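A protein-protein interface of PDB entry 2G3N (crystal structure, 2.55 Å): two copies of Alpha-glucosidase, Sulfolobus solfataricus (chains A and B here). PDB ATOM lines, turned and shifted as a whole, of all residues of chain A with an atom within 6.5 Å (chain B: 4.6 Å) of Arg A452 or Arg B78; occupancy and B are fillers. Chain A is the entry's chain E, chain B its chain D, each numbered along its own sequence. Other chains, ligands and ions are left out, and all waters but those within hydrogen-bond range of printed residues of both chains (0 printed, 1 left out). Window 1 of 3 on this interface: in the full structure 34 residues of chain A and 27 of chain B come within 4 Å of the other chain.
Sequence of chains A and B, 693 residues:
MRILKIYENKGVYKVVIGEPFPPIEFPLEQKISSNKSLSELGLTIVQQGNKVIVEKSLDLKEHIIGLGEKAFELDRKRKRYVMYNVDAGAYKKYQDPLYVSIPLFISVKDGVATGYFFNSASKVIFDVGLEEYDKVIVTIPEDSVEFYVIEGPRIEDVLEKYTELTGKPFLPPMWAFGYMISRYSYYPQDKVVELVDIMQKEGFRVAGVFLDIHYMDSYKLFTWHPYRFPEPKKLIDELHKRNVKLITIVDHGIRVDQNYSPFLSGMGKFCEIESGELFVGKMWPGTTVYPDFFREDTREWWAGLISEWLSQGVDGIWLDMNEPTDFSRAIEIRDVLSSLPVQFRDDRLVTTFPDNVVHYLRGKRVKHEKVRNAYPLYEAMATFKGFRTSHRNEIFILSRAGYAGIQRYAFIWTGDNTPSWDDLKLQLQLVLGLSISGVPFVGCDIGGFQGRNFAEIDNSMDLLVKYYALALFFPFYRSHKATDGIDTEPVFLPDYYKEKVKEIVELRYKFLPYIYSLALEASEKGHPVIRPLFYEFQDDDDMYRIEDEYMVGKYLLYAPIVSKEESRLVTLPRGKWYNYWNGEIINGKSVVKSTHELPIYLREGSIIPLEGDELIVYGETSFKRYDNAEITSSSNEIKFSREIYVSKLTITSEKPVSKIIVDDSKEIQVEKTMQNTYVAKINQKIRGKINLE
No position is printed for both chains.
NH1 of Arg B76 lies within hydrogen-bond range of O of Phe B72 (3.1 Å).
O of Glu B73 is in hydrogen-bond range of NH1 of Arg B76, 2.8 Å away.
The side-chain hydroxyl (OH) of Tyr B94 lies within hydrogen-bond range of the side-chain carboxylate (OE2) of Glu B73 (2.7 Å).
The backbone NH of Arg B78 lies within hydrogen-bond range of the backbone carbonyl oxygen of Val B128 (2.7 Å).
The guanidinium group of Arg A452 lies close to the backbone carbonyl oxygen of Asp A484, 3.0 Å away.
The side-chain carboxylate (OD2) of Asp A484 lies within hydrogen-bond range of the backbone NH (N) of Asn A453, 3.3 Å away.
OE1 of Glu B73 is in salt-bridge range of NH2 of Arg A452, at 2.9 Å.
The guanidinium group (NH1) of Arg A452 is in hydrogen-bond range of the backbone carbonyl oxygen (O) of Lys B77.
The guanidinium group (NH1) of Arg A452 sits at hydrogen-bond distance from the backbone carbonyl oxygen (O) of Arg B78 (3.2 Å).
The side-chain carboxylate (OD2) of Asp A487 is in salt-bridge range of the guanidinium group (NE) of Arg B78, 3.2 Å away.
The backbone carbonyl oxygen of Arg A452 is in hydrogen-bond range of the side-chain amino group of Lys B79.
The side-chain carboxylate (OD2) of Asp A484 is in salt-bridge range of the side-chain amino group (NZ) of Lys B79 (3.0 Å).
The side-chain hydroxyl of Tyr B94 is in hydrogen-bond range of the side-chain amide nitrogen of Asn A459, at 2.8 Å.
OH of Tyr B133 lies within hydrogen-bond range of OD1 of Asp A487 (3.3 Å).
The backbone carbonyl oxygen of Arg B78 sits close to the backbone carbonyl oxygen of Asp A484, at 3.2 Å.
Of the 16 printed residues of chain A, 10 touch a printed residue of chain B.
Hydrophobic or aromatic side chains of chain A that line the printed part of chain B: Ile A486.
Hydrophobic or aromatic side chains of chain B within 4 Å of the printed part of chain A: Phe B72, Tyr B94, Leu B130 and Tyr B133.
Among the printed residues, 20 pairs touch across the chains.
Among the printed residues, Asp or Glu carboxylates within 4 Å of a Lys or Arg side-chain nitrogen of the other chain: Arg A452 with Glu B73 (2.9 Å), Asp A484 with Lys B79 (3.0 Å) and Asp A487 with Arg B78 (3.2 Å).
Arg B78 touches Arg A183 (CG to NH2, 3.4 Å).
CE1 of Tyr B133 touches NE of Arg A183, 3.8 Å away.
CD2 of Phe B72 touches NE of Arg A452, 3.9 Å away.
CZ of Tyr B94 touches CG of Arg A452, at 3.4 Å.
Phe A454 touches Tyr B94 (O to CD2, 3.7 Å).
Ile A457 touches Tyr B94.
Thr A483 touches Arg B78 (O to CB, 3.8 Å).
CG2 of Thr A483 touches CD2 of Leu B130, at 3.3 Å.
N of Asp A484 touches CD2 of Leu B130 (3.9 Å).
Ile A486 touches Glu B73 (CG2 to OE1, 3.8 Å).
Of chain B, only Phe B72, Glu B73, Lys B77, Arg B78, Lys B79 and Tyr B94 come within 4 Å of Arg A452.
Arg B78 touches just these residues of chain A: Arg A183 (3.4 Å), Arg A452 (3.2 Å), Thr A483 (3.8 Å), Asp A484 (3.2 Å), Gly A485 (3.4 Å) and Asp A487 (3.2 Å).
Of the printed residues of chain B, Ile A486 touches Glu B73 (3.8 Å).
Of the printed residues of chain B, Arg A183 touches Arg B78 and Tyr B133.
Of the printed residues of chain B, Ile A457 touches Tyr B94.
Of the printed residues of chain A, Glu B73 touches Arg A452 (2.9 Å) and Ile A486 (3.8 Å).
Of the printed residues of chain A, Phe B72 touches Arg A452 (3.9 Å).
Gln A450 touches none of the printed residues of chain B.
Asn A453 touches none of the printed residues of chain B.
The nearest residue of chain B that does not touch Arg A452 is Tyr B81 (4.3 Å).
The nearest printed residue of chain B that does not touch Gly A485 is Lys B77 (5.2 Å).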
ATOM      1  N   ARG A 183     -27.519 -11.241  -4.495  1.00  0.00           N
ATOM      2  CA  ARG A 183     -28.027 -12.461  -5.070  1.00  0.00           C
ATOM      3  C   ARG A 183     -28.845 -13.145  -3.998  1.00  0.00           C
ATOM      4  O   ARG A 183     -28.753 -12.817  -2.820  1.00  0.00           O
ATOM      5  CB  ARG A 183     -26.889 -13.383  -5.533  1.00  0.00           C
ATOM      6  CG  ARG A 183     -27.400 -14.592  -6.339  1.00  0.00           C
ATOM      7  CD  ARG A 183     -26.310 -15.591  -6.729  1.00  0.00           C
ATOM      8  NE  ARG A 183     -26.891 -16.808  -7.298  1.00  0.00           N
ATOM      9  CZ  ARG A 183     -27.202 -16.980  -8.583  1.00  0.00           C
ATOM     10  NH1 ARG A 183     -26.985 -16.015  -9.468  1.00  0.00           N
ATOM     11  NH2 ARG A 183     -27.749 -18.121  -8.986  1.00  0.00           N
ATOM     12  N   GLN A 450     -35.905 -12.721 -11.646  1.00  0.00           N
ATOM     13  CA  GLN A 450     -36.252 -14.086 -12.049  1.00  0.00           C
ATOM     14  C   GLN A 450     -35.102 -14.868 -12.692  1.00  0.00           C
ATOM     15  O   GLN A 450     -34.371 -14.355 -13.537  1.00  0.00           O
ATOM     16  CB  GLN A 450     -37.460 -14.063 -12.976  1.00  0.00           C
ATOM     17  CG  GLN A 450     -38.697 -13.357 -12.403  1.00  0.00           C
ATOM     18  CD  GLN A 450     -39.241 -14.003 -11.141  1.00  0.00           C
ATOM     19  OE1 GLN A 450     -39.104 -15.212 -10.940  1.00  0.00           O
ATOM     20  NE2 GLN A 450     -39.889 -13.203 -10.293  1.00  0.00           N
ATOM     21  N   GLY A 451     -34.955 -16.123 -12.276  1.00  0.00           N
ATOM     22  CA  GLY A 451     -33.878 -16.958 -12.779  1.00  0.00           C
ATOM     23  C   GLY A 451     -34.201 -17.812 -13.988  1.00  0.00           C
ATOM     24  O   GLY A 451     -34.084 -17.348 -15.115  1.00  0.00           O
ATOM     25  N   ARG A 452     -34.585 -19.064 -13.759  1.00  0.00           N
ATOM     26  CA  ARG A 452     -34.925 -19.968 -14.855  1.00  0.00           C
ATOM     27  C   ARG A 452     -36.035 -20.921 -14.440  1.00  0.00           C
ATOM     28  O   ARG A 452     -36.003 -22.112 -14.758  1.00  0.00           O
ATOM     29  CB  ARG A 452     -33.701 -20.777 -15.290  1.00  0.00           C
ATOM     30  CG  ARG A 452     -32.592 -19.953 -15.886  1.00  0.00           C
ATOM     31  CD  ARG A 452     -31.328 -20.198 -15.134  1.00  0.00           C
ATOM     32  NE  ARG A 452     -30.371 -20.985 -15.895  1.00  0.00           N
ATOM     33  CZ  ARG A 452     -29.360 -21.661 -15.361  1.00  0.00           C
ATOM     34  NH1 ARG A 452     -29.169 -21.663 -14.048  1.00  0.00           N
ATOM     35  NH2 ARG A 452     -28.528 -22.322 -16.155  1.00  0.00           N
ATOM     36  N   ASN A 453     -37.026 -20.398 -13.730  1.00  0.00           N
ATOM     37  CA  ASN A 453     -38.129 -21.234 -13.285  1.00  0.00           C
ATOM     38  C   ASN A 453     -39.306 -21.223 -14.254  1.00  0.00           C
ATOM     39  O   ASN A 453     -40.321 -21.855 -14.000  1.00  0.00           O
ATOM     40  CB  ASN A 453     -38.565 -20.842 -11.867  1.00  0.00           C
ATOM     41  CG  ASN A 453     -38.840 -19.356 -11.722  1.00  0.00           C
ATOM     42  OD1 ASN A 453     -37.997 -18.511 -12.043  1.00  0.00           O
ATOM     43  ND2 ASN A 453     -40.026 -19.027 -11.222  1.00  0.00           N
ATOM     44  N   PHE A 454     -39.164 -20.503 -15.364  1.00  0.00           N
ATOM     45  CA  PHE A 454     -40.189 -20.480 -16.404  1.00  0.00           C
ATOM     46  C   PHE A 454     -39.614 -19.971 -17.728  1.00  0.00           C
ATOM     47  O   PHE A 454     -38.683 -19.167 -17.747  1.00  0.00           O
ATOM     48  CB  PHE A 454     -41.451 -19.706 -15.961  1.00  0.00           C
ATOM     49  CG  PHE A 454     -41.230 -18.257 -15.665  1.00  0.00           C
ATOM     50  CD1 PHE A 454     -41.332 -17.307 -16.672  1.00  0.00           C
ATOM     51  CD2 PHE A 454     -40.952 -17.834 -14.363  1.00  0.00           C
ATOM     52  CE1 PHE A 454     -41.164 -15.953 -16.396  1.00  0.00           C
ATOM     53  CE2 PHE A 454     -40.780 -16.473 -14.070  1.00  0.00           C
ATOM     54  CZ  PHE A 454     -40.887 -15.532 -15.088  1.00  0.00           C
ATOM     55  N   ALA A 455     -40.165 -20.476 -18.828  1.00  0.00           N
ATOM     56  CA  ALA A 455     -39.708 -20.177 -20.188  1.00  0.00           C
ATOM     57  C   ALA A 455     -39.561 -18.732 -20.666  1.00  0.00           C
ATOM     58  O   ALA A 455     -38.624 -18.412 -21.403  1.00  0.00           O
ATOM     59  CB  ALA A 455     -40.589 -20.940 -21.186  1.00  0.00           C
ATOM     60  N   ILE A 457     -38.220 -16.096 -19.847  1.00  0.00           N
ATOM     61  CA  ILE A 457     -37.146 -15.337 -19.222  1.00  0.00           C
ATOM     62  C   ILE A 457     -36.004 -15.243 -20.226  1.00  0.00           C
ATOM     63  O   ILE A 457     -35.594 -16.252 -20.805  1.00  0.00           O
ATOM     64  CB  ILE A 457     -36.632 -16.024 -17.945  1.00  0.00           C
ATOM     65  CG1 ILE A 457     -37.767 -16.146 -16.928  1.00  0.00           C
ATOM     66  CG2 ILE A 457     -35.479 -15.220 -17.341  1.00  0.00           C
ATOM     67  CD1 ILE A 457     -37.358 -16.816 -15.622  1.00  0.00           C
ATOM     68  N   ASN A 459     -32.173 -14.443 -20.659  1.00  0.00           N
ATOM     69  CA  ASN A 459     -30.887 -14.236 -20.003  1.00  0.00           C
ATOM     70  C   ASN A 459     -29.727 -13.895 -20.938  1.00  0.00           C
ATOM     71  O   ASN A 459     -28.568 -14.119 -20.594  1.00  0.00           O
ATOM     72  CB  ASN A 459     -30.527 -15.463 -19.166  1.00  0.00           C
ATOM     73  CG  ASN A 459     -31.451 -15.639 -17.983  1.00  0.00           C
ATOM     74  OD1 ASN A 459     -31.540 -14.767 -17.117  1.00  0.00           O
ATOM     75  ND2 ASN A 459     -32.150 -16.767 -17.939  1.00  0.00           N
ATOM     76  N   ALA A 482     -32.208 -14.279  -8.718  1.00  0.00           N
ATOM     77  CA  ALA A 482     -32.783 -15.402  -7.981  1.00  0.00           C
ATOM     78  C   ALA A 482     -31.821 -16.605  -7.893  1.00  0.00           C
ATOM     79  O   ALA A 482     -30.852 -16.710  -8.647  1.00  0.00           O
ATOM     80  CB  ALA A 482     -34.095 -15.826  -8.625  1.00  0.00           C
ATOM     81  N   THR A 483     -32.114 -17.521  -6.977  1.00  0.00           N
ATOM     82  CA  THR A 483     -31.269 -18.689  -6.752  1.00  0.00           C
ATOM     83  C   THR A 483     -30.895 -19.520  -7.962  1.00  0.00           C
ATOM     84  O   THR A 483     -29.726 -19.864  -8.137  1.00  0.00           O
ATOM     85  CB  THR A 483     -31.900 -19.613  -5.730  1.00  0.00           C
ATOM     86  OG1 THR A 483     -32.598 -18.821  -4.759  1.00  0.00           O
ATOM     87  CG2 THR A 483     -30.822 -20.431  -5.021  1.00  0.00           C
ATOM     88  N   ASP A 484     -31.874 -19.840  -8.800  1.00  0.00           N
ATOM     89  CA  ASP A 484     -31.613 -20.661  -9.977  1.00  0.00           C
ATOM     90  C   ASP A 484     -31.279 -19.883 -11.247  1.00  0.00           C
ATOM     91  O   ASP A 484     -31.284 -20.446 -12.337  1.00  0.00           O
ATOM     92  CB  ASP A 484     -32.802 -21.600 -10.234  1.00  0.00           C
ATOM     93  CG  ASP A 484     -34.013 -20.883 -10.828  1.00  0.00           C
ATOM     94  OD1 ASP A 484     -34.236 -19.686 -10.529  1.00  0.00           O
ATOM     95  OD2 ASP A 484     -34.763 -21.535 -11.589  1.00  0.00           O
ATOM     96  N   GLY A 485     -30.998 -18.591 -11.107  1.00  0.00           N
ATOM     97  CA  GLY A 485     -30.642 -17.797 -12.270  1.00  0.00           C
ATOM     98  C   GLY A 485     -29.157 -17.922 -12.541  1.00  0.00           C
ATOM     99  O   GLY A 485     -28.384 -18.239 -11.638  1.00  0.00           O
ATOM    100  N   ILE A 486     -28.747 -17.686 -13.781  1.00  0.00           N
ATOM    101  CA  ILE A 486     -27.330 -17.767 -14.126  1.00  0.00           C
ATOM    102  C   ILE A 486     -26.579 -16.709 -13.318  1.00  0.00           C
ATOM    103  O   ILE A 486     -27.190 -15.750 -12.842  1.00  0.00           O
ATOM    104  CB  ILE A 486     -27.102 -17.481 -15.628  1.00  0.00           C
ATOM    105  CG1 ILE A 486     -27.680 -16.106 -15.979  1.00  0.00           C
ATOM    106  CG2 ILE A 486     -27.757 -18.569 -16.473  1.00  0.00           C
ATOM    107  CD1 ILE A 486     -27.461 -15.697 -17.420  1.00  0.00           C
ATOM    108  N   ASP A 487     -25.269 -16.892 -13.150  1.00  0.00           N
ATOM    109  CA  ASP A 487     -24.458 -15.919 -12.417  1.00  0.00           C
ATOM    110  C   ASP A 487     -24.386 -14.667 -13.289  1.00  0.00           C
ATOM    111  O   ASP A 487     -23.960 -14.735 -14.444  1.00  0.00           O
ATOM    112  CB  ASP A 487     -23.048 -16.466 -12.168  1.00  0.00           C
ATOM    113  CG  ASP A 487     -23.015 -17.561 -11.099  1.00  0.00           C
ATOM    114  OD1 ASP A 487     -23.394 -17.281  -9.937  1.00  0.00           O
ATOM    115  OD2 ASP A 487     -22.605 -18.700 -11.422  1.00  0.00           O
ATOM    116  N   PHE A 492     -18.030 -12.678 -14.570  1.00  0.00           N
ATOM    117  CA  PHE A 492     -18.317 -13.954 -15.220  1.00  0.00           C
ATOM    118  C   PHE A 492     -18.712 -13.800 -16.680  1.00  0.00           C
ATOM    119  O   PHE A 492     -19.081 -14.778 -17.329  1.00  0.00           O
ATOM    120  CB  PHE A 492     -19.433 -14.702 -14.486  1.00  0.00           C
ATOM    121  CG  PHE A 492     -19.096 -15.051 -13.068  1.00  0.00           C
ATOM    122  CD1 PHE A 492     -18.004 -15.863 -12.782  1.00  0.00           C
ATOM    123  CD2 PHE A 492     -19.865 -14.559 -12.016  1.00  0.00           C
ATOM    124  CE1 PHE A 492     -17.676 -16.183 -11.468  1.00  0.00           C
ATOM    125  CE2 PHE A 492     -19.551 -14.870 -10.697  1.00  0.00           C
ATOM    126  CZ  PHE A 492     -18.450 -15.686 -10.419  1.00  0.00           C
ATOM    127  N   LEU B  58     -17.416 -26.622  -5.125  1.00  0.00           N
ATOM    128  CA  LEU B  58     -17.577 -25.914  -6.383  1.00  0.00           C
ATOM    129  C   LEU B  58     -17.017 -24.509  -6.207  1.00  0.00           C
ATOM    130  O   LEU B  58     -17.532 -23.727  -5.404  1.00  0.00           O
ATOM    131  CB  LEU B  58     -19.061 -25.835  -6.742  1.00  0.00           C
ATOM    132  CG  LEU B  58     -19.427 -25.178  -8.071  1.00  0.00           C
ATOM    133  CD1 LEU B  58     -19.007 -26.078  -9.235  1.00  0.00           C
ATOM    134  CD2 LEU B  58     -20.921 -24.929  -8.107  1.00  0.00           C
ATOM    135  N   PHE B  72     -30.962 -25.895 -21.010  1.00  0.00           N
ATOM    136  CA  PHE B  72     -30.284 -24.855 -20.245  1.00  0.00           C
ATOM    137  C   PHE B  72     -28.933 -24.480 -20.850  1.00  0.00           C
ATOM    138  O   PHE B  72     -28.443 -25.137 -21.777  1.00  0.00           O
ATOM    139  CB  PHE B  72     -30.041 -25.313 -18.802  1.00  0.00           C
ATOM    140  CG  PHE B  72     -31.290 -25.458 -17.987  1.00  0.00           C
ATOM    141  CD1 PHE B  72     -32.091 -26.584 -18.115  1.00  0.00           C
ATOM    142  CD2 PHE B  72     -31.675 -24.458 -17.103  1.00  0.00           C
ATOM    143  CE1 PHE B  72     -33.268 -26.713 -17.370  1.00  0.00           C
ATOM    144  CE2 PHE B  72     -32.851 -24.579 -16.356  1.00  0.00           C
ATOM    145  CZ  PHE B  72     -33.645 -25.710 -16.494  1.00  0.00           C
ATOM    146  N   GLU B  73     -28.338 -23.421 -20.310  1.00  0.00           N
ATOM    147  CA  GLU B  73     -27.029 -22.971 -20.747  1.00  0.00           C
ATOM    148  C   GLU B  73     -26.034 -24.133 -20.576  1.00  0.00           C
ATOM    149  O   GLU B  73     -26.193 -24.973 -19.682  1.00  0.00           O
ATOM    150  CB  GLU B  73     -26.574 -21.774 -19.900  1.00  0.00           C
ATOM    151  CG  GLU B  73     -27.341 -20.445 -20.128  1.00  0.00           C
ATOM    152  CD  GLU B  73     -28.803 -20.482 -19.675  1.00  0.00           C
ATOM    153  OE1 GLU B  73     -29.147 -21.266 -18.756  1.00  0.00           O
ATOM    154  OE2 GLU B  73     -29.610 -19.707 -20.232  1.00  0.00           O
ATOM    155  N   ASP B  75     -23.008 -24.167 -19.378  1.00  0.00           N
ATOM    156  CA  ASP B  75     -22.369 -24.186 -18.057  1.00  0.00           C
ATOM    157  C   ASP B  75     -23.571 -24.389 -17.130  1.00  0.00           C
ATOM    158  O   ASP B  75     -24.402 -23.494 -16.980  1.00  0.00           O
ATOM    159  CB  ASP B  75     -21.681 -22.856 -17.733  1.00  0.00           C
ATOM    160  CG  ASP B  75     -20.743 -22.958 -16.506  1.00  0.00           C
ATOM    161  OD1 ASP B  75     -21.108 -23.619 -15.502  1.00  0.00           O
ATOM    162  OD2 ASP B  75     -19.637 -22.366 -16.541  1.00  0.00           O
ATOM    163  N   ARG B  76     -23.645 -25.564 -16.511  1.00  0.00           N
ATOM    164  CA  ARG B  76     -24.777 -25.946 -15.676  1.00  0.00           C
ATOM    165  C   ARG B  76     -24.960 -25.407 -14.262  1.00  0.00           C
ATOM    166  O   ARG B  76     -25.923 -25.777 -13.592  1.00  0.00           O
ATOM    167  CB  ARG B  76     -24.836 -27.472 -15.607  1.00  0.00           C
ATOM    168  CG  ARG B  76     -24.646 -28.192 -16.930  1.00  0.00           C
ATOM    169  CD  ARG B  76     -25.687 -27.809 -17.969  1.00  0.00           C
ATOM    170  NE  ARG B  76     -25.755 -28.819 -19.025  1.00  0.00           N
ATOM    171  CZ  ARG B  76     -26.365 -28.670 -20.198  1.00  0.00           C
ATOM    172  NH1 ARG B  76     -26.981 -27.536 -20.510  1.00  0.00           N
ATOM    173  NH2 ARG B  76     -26.368 -29.675 -21.061  1.00  0.00           N
ATOM    174  N   LYS B  77     -24.075 -24.546 -13.788  1.00  0.00           N
ATOM    175  CA  LYS B  77     -24.215 -24.032 -12.424  1.00  0.00           C
ATOM    176  C   LYS B  77     -25.537 -23.317 -12.104  1.00  0.00           C
ATOM    177  O   LYS B  77     -26.186 -22.757 -12.976  1.00  0.00           O
ATOM    178  CB  LYS B  77     -23.041 -23.106 -12.098  1.00  0.00           C
ATOM    179  CG  LYS B  77     -21.698 -23.812 -12.129  1.00  0.00           C
ATOM    180  CD  LYS B  77     -20.532 -22.831 -12.207  1.00  0.00           C
ATOM    181  CE  LYS B  77     -20.343 -22.058 -10.922  1.00  0.00           C
ATOM    182  NZ  LYS B  77     -19.186 -21.123 -11.052  1.00  0.00           N
ATOM    183  N   ARG B  78     -25.915 -23.377 -10.829  1.00  0.00           N
ATOM    184  CA  ARG B  78     -27.115 -22.746 -10.276  1.00  0.00           C
ATOM    185  C   ARG B  78     -28.433 -23.366 -10.714  1.00  0.00           C
ATOM    186  O   ARG B  78     -29.388 -22.666 -11.042  1.00  0.00           O
ATOM    187  CB  ARG B  78     -27.126 -21.244 -10.590  1.00  0.00           C
ATOM    188  CG  ARG B  78     -25.785 -20.553 -10.387  1.00  0.00           C
ATOM    189  CD  ARG B  78     -25.155 -20.883  -9.038  1.00  0.00           C
ATOM    190  NE  ARG B  78     -23.778 -20.395  -8.986  1.00  0.00           N
ATOM    191  CZ  ARG B  78     -22.867 -20.798  -8.105  1.00  0.00           C
ATOM    192  NH1 ARG B  78     -23.178 -21.704  -7.197  1.00  0.00           N
ATOM    193  NH2 ARG B  78     -21.648 -20.287  -8.126  1.00  0.00           N
ATOM    194  N   LYS B  79     -28.493 -24.688 -10.704  1.00  0.00           N
ATOM    195  CA  LYS B  79     -29.711 -25.372 -11.098  1.00  0.00           C
ATOM    196  C   LYS B  79     -29.709 -26.763 -10.505  1.00  0.00           C
ATOM    197  O   LYS B  79     -28.654 -27.352 -10.311  1.00  0.00           O
ATOM    198  CB  LYS B  79     -29.802 -25.455 -12.630  1.00  0.00           C
ATOM    199  CG  LYS B  79     -31.162 -25.901 -13.129  1.00  0.00           C
ATOM    200  CD  LYS B  79     -32.227 -24.876 -12.751  1.00  0.00           C
ATOM    201  CE  LYS B  79     -33.639 -25.425 -12.935  1.00  0.00           C
ATOM    202  NZ  LYS B  79     -34.677 -24.382 -12.613  1.00  0.00           N
ATOM    203  N   TYR B  81     -30.816 -30.332 -11.394  1.00  0.00           N
ATOM    204  CA  TYR B  81     -31.279 -31.166 -12.505  1.00  0.00           C
ATOM    205  C   TYR B  81     -31.788 -32.527 -12.078  1.00  0.00           C
ATOM    206  O   TYR B  81     -31.286 -33.125 -11.127  1.00  0.00           O
ATOM    207  CB  TYR B  81     -30.166 -31.368 -13.534  1.00  0.00           C
ATOM    208  CG  TYR B  81     -29.572 -30.081 -14.043  1.00  0.00           C
ATOM    209  CD1 TYR B  81     -28.559 -29.434 -13.337  1.00  0.00           C
ATOM    210  CD2 TYR B  81     -30.037 -29.494 -15.222  1.00  0.00           C
ATOM    211  CE1 TYR B  81     -28.022 -28.244 -13.787  1.00  0.00           C
ATOM    212  CE2 TYR B  81     -29.510 -28.296 -15.681  1.00  0.00           C
ATOM    213  CZ  TYR B  81     -28.501 -27.676 -14.961  1.00  0.00           C
ATOM    214  OH  TYR B  81     -27.963 -26.492 -15.413  1.00  0.00           O
ATOM    215  N   TYR B  94     -35.753 -24.103 -20.360  1.00  0.00           N
ATOM    216  CA  TYR B  94     -35.740 -24.238 -18.913  1.00  0.00           C
ATOM    217  C   TYR B  94     -36.689 -25.311 -18.401  1.00  0.00           C
ATOM    218  O   TYR B  94     -36.965 -25.390 -17.208  1.00  0.00           O
ATOM    219  CB  TYR B  94     -36.009 -22.894 -18.226  1.00  0.00           C
ATOM    220  CG  TYR B  94     -34.996 -21.841 -18.601  1.00  0.00           C
ATOM    221  CD1 TYR B  94     -33.680 -22.190 -18.880  1.00  0.00           C
ATOM    222  CD2 TYR B  94     -35.347 -20.494 -18.674  1.00  0.00           C
ATOM    223  CE1 TYR B  94     -32.732 -21.231 -19.227  1.00  0.00           C
ATOM    224  CE2 TYR B  94     -34.402 -19.518 -19.016  1.00  0.00           C
ATOM    225  CZ  TYR B  94     -33.104 -19.896 -19.290  1.00  0.00           C
ATOM    226  OH  TYR B  94     -32.161 -18.955 -19.635  1.00  0.00           O
ATOM    227  N   VAL B 128     -26.375 -28.600  -8.807  1.00  0.00           N
ATOM    228  CA  VAL B 128     -25.140 -27.893  -9.116  1.00  0.00           C
ATOM    229  C   VAL B 128     -25.071 -26.468  -8.571  1.00  0.00           C
ATOM    230  O   VAL B 128     -25.399 -25.509  -9.258  1.00  0.00           O
ATOM    231  CB  VAL B 128     -24.923 -27.869 -10.647  1.00  0.00           C
ATOM    232  CG1 VAL B 128     -23.547 -27.352 -10.987  1.00  0.00           C
ATOM    233  CG2 VAL B 128     -25.114 -29.259 -11.206  1.00  0.00           C
ATOM    234  N   GLY B 129     -24.636 -26.342  -7.328  1.00  0.00           N
ATOM    235  CA  GLY B 129     -24.502 -25.040  -6.702  1.00  0.00           C
ATOM    236  C   GLY B 129     -25.805 -24.316  -6.464  1.00  0.00           C
ATOM    237  O   GLY B 129     -25.858 -23.091  -6.557  1.00  0.00           O
ATOM    238  N   LEU B 130     -26.854 -25.064  -6.142  1.00  0.00           N
ATOM    239  CA  LEU B 130     -28.172 -24.482  -5.900  1.00  0.00           C
ATOM    240  C   LEU B 130     -28.524 -24.631  -4.421  1.00  0.00           C
ATOM    241  O   LEU B 130     -28.809 -23.653  -3.734  1.00  0.00           O
ATOM    242  CB  LEU B 130     -29.209 -25.179  -6.796  1.00  0.00           C
ATOM    243  CG  LEU B 130     -30.578 -24.558  -7.109  1.00  0.00           C
ATOM    244  CD1 LEU B 130     -31.624 -25.108  -6.184  1.00  0.00           C
ATOM    245  CD2 LEU B 130     -30.500 -23.042  -7.032  1.00  0.00           C
ATOM    246  N   TYR B 133     -24.448 -23.032  -2.584  1.00  0.00           N
ATOM    247  CA  TYR B 133     -23.740 -22.241  -3.588  1.00  0.00           C
ATOM    248  C   TYR B 133     -22.327 -22.745  -3.942  1.00  0.00           C
ATOM    249  O   TYR B 133     -21.876 -22.620  -5.077  1.00  0.00           O
ATOM    250  CB  TYR B 133     -23.660 -20.784  -3.101  1.00  0.00           C
ATOM    251  CG  TYR B 133     -23.211 -19.786  -4.143  1.00  0.00           C
ATOM    252  CD1 TYR B 133     -24.105 -19.285  -5.095  1.00  0.00           C
ATOM    253  CD2 TYR B 133     -21.896 -19.333  -4.175  1.00  0.00           C
ATOM    254  CE1 TYR B 133     -23.700 -18.358  -6.051  1.00  0.00           C
ATOM    255  CE2 TYR B 133     -21.482 -18.403  -5.130  1.00  0.00           C
ATOM    256  CZ  TYR B 133     -22.392 -17.923  -6.058  1.00  0.00           C
ATOM    257  OH  TYR B 133     -21.978 -17.006  -6.989  1.00  0.00           O
